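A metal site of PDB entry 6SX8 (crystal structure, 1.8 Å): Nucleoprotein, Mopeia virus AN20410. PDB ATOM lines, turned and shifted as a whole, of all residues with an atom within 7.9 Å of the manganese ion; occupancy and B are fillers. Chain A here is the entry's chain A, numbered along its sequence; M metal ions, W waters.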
ATOM      1  N   ILE A  25     -10.050  19.080 -15.949  1.00  0.00           N
ATOM      2  CA  ILE A  25     -10.717  19.355 -17.224  1.00  0.00           C
ATOM      3  C   ILE A  25      -9.716  19.140 -18.352  1.00  0.00           C
ATOM      4  O   ILE A  25      -8.515  19.410 -18.198  1.00  0.00           O
ATOM      5  CB  ILE A  25     -11.348  20.778 -17.259  1.00  0.00           C
ATOM      6  CG1 ILE A  25     -12.199  20.977 -18.531  1.00  0.00           C
ATOM      7  CG2 ILE A  25     -10.275  21.881 -17.103  1.00  0.00           C
ATOM      8  CD1 ILE A  25     -12.975  22.310 -18.594  1.00  0.00           C
ATOM      9  N   ASP A  26     -10.183  18.609 -19.488  1.00  0.00           N
ATOM     10  CA  ASP A  26      -9.351  18.404 -20.670  1.00  0.00           C
ATOM     11  C   ASP A  26     -10.246  18.469 -21.912  1.00  0.00           C
ATOM     12  O   ASP A  26     -11.370  17.984 -21.870  1.00  0.00           O
ATOM     13  CB  ASP A  26      -8.636  17.043 -20.638  1.00  0.00           C
ATOM     14  CG  ASP A  26      -7.399  17.003 -21.510  1.00  0.00           C
ATOM     15  OD1 ASP A  26      -6.420  17.705 -21.195  1.00  0.00           O
ATOM     16  OD2 ASP A  26      -7.394  16.278 -22.524  1.00  0.00           O
ATOM     17  N   ILE A  27      -9.740  19.065 -22.991  1.00  0.00           N
ATOM     18  CA  ILE A  27     -10.451  19.137 -24.261  1.00  0.00           C
ATOM     19  C   ILE A  27      -9.538  18.667 -25.383  1.00  0.00           C
ATOM     20  O   ILE A  27      -8.312  18.827 -25.329  1.00  0.00           O
ATOM     21  CB  ILE A  27     -10.982  20.561 -24.577  1.00  0.00           C
ATOM     22  CG1 ILE A  27      -9.824  21.527 -24.853  1.00  0.00           C
ATOM     23  CG2 ILE A  27     -11.864  21.086 -23.454  1.00  0.00           C
ATOM     24  CD1 ILE A  27     -10.289  22.881 -25.426  1.00  0.00           C
ATOM     25  N   GLU A  28     -10.144  18.071 -26.402  1.00  0.00           N
ATOM     26  CA  GLU A  28      -9.516  17.861 -27.702  1.00  0.00           C
ATOM     27  C   GLU A  28     -10.167  18.776 -28.728  1.00  0.00           C
ATOM     28  O   GLU A  28     -11.367  19.049 -28.657  1.00  0.00           O
ATOM     29  CB  GLU A  28      -9.631  16.418 -28.180  1.00  0.00           C
ATOM     30  CG  GLU A  28      -9.167  15.340 -27.181  1.00  0.00           C
ATOM     31  CD  GLU A  28      -7.777  15.596 -26.614  1.00  0.00           C
ATOM     32  OE1 GLU A  28      -6.916  16.080 -27.381  1.00  0.00           O
ATOM     33  OE2 GLU A  28      -7.532  15.295 -25.419  1.00  0.00           O
ATOM     34  N   GLY A  29      -9.379  19.237 -29.692  1.00  0.00           N
ATOM     35  CA  GLY A  29      -9.798  20.303 -30.576  1.00  0.00           C
ATOM     36  C   GLY A  29      -9.414  21.677 -30.055  1.00  0.00           C
ATOM     37  O   GLY A  29      -9.232  21.899 -28.854  1.00  0.00           O
ATOM     38  N   GLU A  36     -14.055  17.210 -28.166  1.00  0.00           N
ATOM     39  CA  GLU A  36     -14.247  16.295 -27.047  1.00  0.00           C
ATOM     40  C   GLU A  36     -13.874  17.017 -25.757  1.00  0.00           C
ATOM     41  O   GLU A  36     -12.869  17.722 -25.725  1.00  0.00           O
ATOM     42  CB  GLU A  36     -13.403  15.027 -27.228  1.00  0.00           C
ATOM     43  CG  GLU A  36     -13.792  13.883 -26.283  1.00  0.00           C
ATOM     44  CD  GLU A  36     -12.774  12.759 -26.267  1.00  0.00           C
ATOM     45  OE1 GLU A  36     -11.588  13.006 -26.579  1.00  0.00           O
ATOM     46  OE2 GLU A  36     -13.174  11.626 -25.926  1.00  0.00           O
ATOM     47  N   SER A  67      -3.456  13.534 -33.703  1.00  0.00           N
ATOM     48  CA  SER A  67      -3.748  13.745 -32.295  1.00  0.00           C
ATOM     49  C   SER A  67      -4.836  12.810 -31.767  1.00  0.00           C
ATOM     50  O   SER A  67      -4.546  11.923 -30.974  1.00  0.00           O
ATOM     51  CB  SER A  67      -4.141  15.189 -32.025  1.00  0.00           C
ATOM     52  OG  SER A  67      -4.473  15.346 -30.654  1.00  0.00           O
ATOM     53  N   HIS A  68      -6.096  13.015 -32.191  1.00  0.00           N
ATOM     54  CA  HIS A  68      -7.184  12.296 -31.543  1.00  0.00           C
ATOM     55  C   HIS A  68      -7.792  11.154 -32.363  1.00  0.00           C
ATOM     56  O   HIS A  68      -8.513  10.337 -31.800  1.00  0.00           O
ATOM     57  CB  HIS A  68      -8.306  13.278 -31.108  1.00  0.00           C
ATOM     58  CG  HIS A  68      -8.854  14.129 -32.212  1.00  0.00           C
ATOM     59  ND1 HIS A  68      -9.445  13.601 -33.344  1.00  0.00           N
ATOM     60  CD2 HIS A  68      -8.952  15.471 -32.336  1.00  0.00           C
ATOM     61  CE1 HIS A  68      -9.847  14.582 -34.124  1.00  0.00           C
ATOM     62  NE2 HIS A  68      -9.569  15.732 -33.532  1.00  0.00           N
ATOM     63  N   GLN A  99      -3.733  20.286 -17.515  1.00  0.00           N
ATOM     64  CA  GLN A  99      -2.369  20.150 -18.004  1.00  0.00           C
ATOM     65  C   GLN A  99      -2.271  20.992 -19.269  1.00  0.00           C
ATOM     66  O   GLN A  99      -2.682  20.571 -20.354  1.00  0.00           O
ATOM     67  CB  GLN A  99      -2.019  18.683 -18.260  1.00  0.00           C
ATOM     68  CG  GLN A  99      -0.787  18.446 -19.115  1.00  0.00           C
ATOM     69  CD  GLN A  99       0.520  18.725 -18.378  1.00  0.00           C
ATOM     70  OE1 GLN A  99       0.519  19.164 -17.224  1.00  0.00           O
ATOM     71  NE2 GLN A  99       1.632  18.452 -19.043  1.00  0.00           N
ATOM     72  N   ILE A 104      -7.853  26.013 -22.658  1.00  0.00           N
ATOM     73  CA  ILE A 104      -9.039  25.924 -21.803  1.00  0.00           C
ATOM     74  C   ILE A 104      -9.429  27.292 -21.245  1.00  0.00           C
ATOM     75  O   ILE A 104     -10.619  27.595 -21.138  1.00  0.00           O
ATOM     76  CB  ILE A 104      -8.775  24.880 -20.707  1.00  0.00           C
ATOM     77  CG1 ILE A 104      -8.574  23.513 -21.381  1.00  0.00           C
ATOM     78  CG2 ILE A 104      -9.906  24.861 -19.687  1.00  0.00           C
ATOM     79  CD1 ILE A 104      -8.734  22.329 -20.504  1.00  0.00           C
ATOM     80  N   ARG A 129       2.378  11.700 -19.364  1.00  0.00           N
ATOM     81  CA  ARG A 129       1.881  10.487 -20.002  1.00  0.00           C
ATOM     82  C   ARG A 129       2.637   9.241 -19.553  1.00  0.00           C
ATOM     83  O   ARG A 129       2.685   8.245 -20.277  1.00  0.00           O
ATOM     84  CB  ARG A 129       1.933  10.634 -21.517  1.00  0.00           C
ATOM     85  CG  ARG A 129       1.224  11.890 -21.977  1.00  0.00           C
ATOM     86  CD  ARG A 129       0.902  11.882 -23.464  1.00  0.00           C
ATOM     87  NE  ARG A 129      -0.034  12.966 -23.749  1.00  0.00           N
ATOM     88  CZ  ARG A 129      -1.352  12.799 -23.838  1.00  0.00           C
ATOM     89  NH1 ARG A 129      -1.890  11.596 -23.687  1.00  0.00           N
ATOM     90  NH2 ARG A 129      -2.137  13.839 -24.085  1.00  0.00           N
ATOM     91  N   HIS A 165      -5.046  10.683 -28.517  1.00  0.00           N
ATOM     92  CA  HIS A 165      -5.325  11.540 -27.369  1.00  0.00           C
ATOM     93  C   HIS A 165      -6.830  11.629 -27.159  1.00  0.00           C
ATOM     94  O   HIS A 165      -7.572  12.033 -28.062  1.00  0.00           O
ATOM     95  CB  HIS A 165      -4.727  12.934 -27.580  1.00  0.00           C
ATOM     96  CG  HIS A 165      -3.226  12.953 -27.544  1.00  0.00           C
ATOM     97  ND1 HIS A 165      -2.509  14.135 -27.490  1.00  0.00           N
ATOM     98  CD2 HIS A 165      -2.313  11.953 -27.552  1.00  0.00           C
ATOM     99  CE1 HIS A 165      -1.213  13.852 -27.464  1.00  0.00           C
ATOM    100  NE2 HIS A 165      -1.075  12.540 -27.499  1.00  0.00           N
ATOM    101  N   CYS A 166      -7.274  11.261 -25.954  1.00  0.00           N
ATOM    102  CA  CYS A 166      -8.678  11.247 -25.585  1.00  0.00           C
ATOM    103  C   CYS A 166      -8.845  12.149 -24.370  1.00  0.00           C
ATOM    104  O   CYS A 166      -8.094  12.022 -23.383  1.00  0.00           O
ATOM    105  CB  CYS A 166      -9.145   9.808 -25.271  1.00  0.00           C
ATOM    106  SG  CYS A 166     -10.671   9.649 -24.300  1.00  0.00           S
ATOM    107  N   ALA A 167      -9.811  13.074 -24.426  1.00  0.00           N
ATOM    108  CA  ALA A 167      -9.998  14.025 -23.332  1.00  0.00           C
ATOM    109  C   ALA A 167     -10.193  13.301 -21.996  1.00  0.00           C
ATOM    110  O   ALA A 167      -9.604  13.686 -20.973  1.00  0.00           O
ATOM    111  CB  ALA A 167     -11.187  14.945 -23.609  1.00  0.00           C
ATOM    112  N   LEU A 168     -11.009  12.257 -22.012  1.00  0.00           N
ATOM    113  CA  LEU A 168     -11.297  11.506 -20.796  1.00  0.00           C
ATOM    114  C   LEU A 168     -10.050  10.808 -20.286  1.00  0.00           C
ATOM    115  O   LEU A 168      -9.664  10.979 -19.120  1.00  0.00           O
ATOM    116  CB  LEU A 168     -12.418  10.502 -21.031  1.00  0.00           C
ATOM    117  CG  LEU A 168     -12.776   9.612 -19.823  1.00  0.00           C
ATOM    118  CD1 LEU A 168     -13.200  10.469 -18.637  1.00  0.00           C
ATOM    119  CD2 LEU A 168     -13.881   8.633 -20.212  1.00  0.00           C
ATOM    120  N   LEU A 169      -9.408  10.001 -21.131  1.00  0.00           N
ATOM    121  CA  LEU A 169      -8.295   9.194 -20.624  1.00  0.00           C
ATOM    122  C   LEU A 169      -7.100  10.058 -20.268  1.00  0.00           C
ATOM    123  O   LEU A 169      -6.349   9.733 -19.346  1.00  0.00           O
ATOM    124  CB  LEU A 169      -7.918   8.130 -21.667  1.00  0.00           C
ATOM    125  CG  LEU A 169      -8.548   6.746 -21.419  1.00  0.00           C
ATOM    126  CD1 LEU A 169     -10.055   6.825 -21.168  1.00  0.00           C
ATOM    127  CD2 LEU A 169      -8.261   5.794 -22.583  1.00  0.00           C
ATOM    128  N   ASP A 170      -6.937  11.199 -20.945  1.00  0.00           N
ATOM    129  CA  ASP A 170      -5.912  12.157 -20.550  1.00  0.00           C
ATOM    130  C   ASP A 170      -6.138  12.646 -19.128  1.00  0.00           C
ATOM    131  O   ASP A 170      -5.177  12.795 -18.363  1.00  0.00           O
ATOM    132  CB  ASP A 170      -5.888  13.341 -21.520  1.00  0.00           C
ATOM    133  CG  ASP A 170      -5.175  13.041 -22.818  1.00  0.00           C
ATOM    134  OD1 ASP A 170      -4.795  11.882 -23.053  1.00  0.00           O
ATOM    135  OD2 ASP A 170      -4.990  13.971 -23.620  1.00  0.00           O
ATOM    136  N   CYS A 171      -7.387  12.940 -18.755  1.00  0.00           N
ATOM    137  CA  CYS A 171      -7.648  13.343 -17.378  1.00  0.00           C
ATOM    138  C   CYS A 171      -7.251  12.241 -16.417  1.00  0.00           C
ATOM    139  O   CYS A 171      -6.644  12.503 -15.358  1.00  0.00           O
ATOM    140  CB  CYS A 171      -9.127  13.654 -17.177  1.00  0.00           C
ATOM    141  SG  CYS A 171      -9.599  15.250 -17.849  1.00  0.00           S
ATOM    142  N   PHE A 174      -3.402  11.965 -16.270  1.00  0.00           N
ATOM    143  CA  PHE A 174      -2.825  13.085 -15.536  1.00  0.00           C
ATOM    144  C   PHE A 174      -3.016  12.918 -14.030  1.00  0.00           C
ATOM    145  O   PHE A 174      -2.091  13.169 -13.248  1.00  0.00           O
ATOM    146  CB  PHE A 174      -3.413  14.408 -16.018  1.00  0.00           C
ATOM    147  CG  PHE A 174      -3.179  14.667 -17.469  1.00  0.00           C
ATOM    148  CD1 PHE A 174      -2.183  13.995 -18.165  1.00  0.00           C
ATOM    149  CD2 PHE A 174      -3.986  15.563 -18.169  1.00  0.00           C
ATOM    150  CE1 PHE A 174      -1.969  14.224 -19.523  1.00  0.00           C
ATOM    151  CE2 PHE A 174      -3.788  15.787 -19.528  1.00  0.00           C
ATOM    152  CZ  PHE A 174      -2.776  15.117 -20.209  1.00  0.00           C
HETATM  153 MN    MN M   1      -5.974  15.969 -24.136  1.00  0.00          MN
HETATM  154  O   HOH W   1      -4.069  16.753 -23.089  1.00  0.00           O
HETATM  155  O   HOH W   2      -5.756  17.978 -25.065  1.00  0.00           O
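The manganese ion is bound by the side-chain carboxylate (OE2) of Glu 28 (2.1 Å), the side-chain carboxylate (OD2) of Asp 26 (2.2 Å), water W2 (2.2 Å), the side-chain carboxylate (OD2) of Asp 170 (2.3 Å) and water W1 (2.3 Å).
The manganese ion has five donor atoms within binding distance.
Ile 27 touches the manganese ion.
Of the 19 residues printed, 4 come within 4 Å of the manganese ion.
The nearest printed residue that does not touch the manganese ion is Arg 129 (4.4 Å).
N of Ala 167 lies close to OE2 of Glu 28 (3.3 Å).
The backbone carbonyl oxygen (O) of Glu 36 is in hydrogen-bond range of the backbone NH (N) of Glu 28 (2.8 Å).
N of Asp 26 lies close to SG of Cys 171, 3.8 Å away.
OD1 of Asp 170 is in salt-bridge range of NH1 of Arg 129, at 3.0 Å.
Water W2 bridges the backbone carbonyl oxygen (O) of Ile 27 (2.7 Å) and the side-chain carboxylate (OE1) of Glu 28 (3.2 Å).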
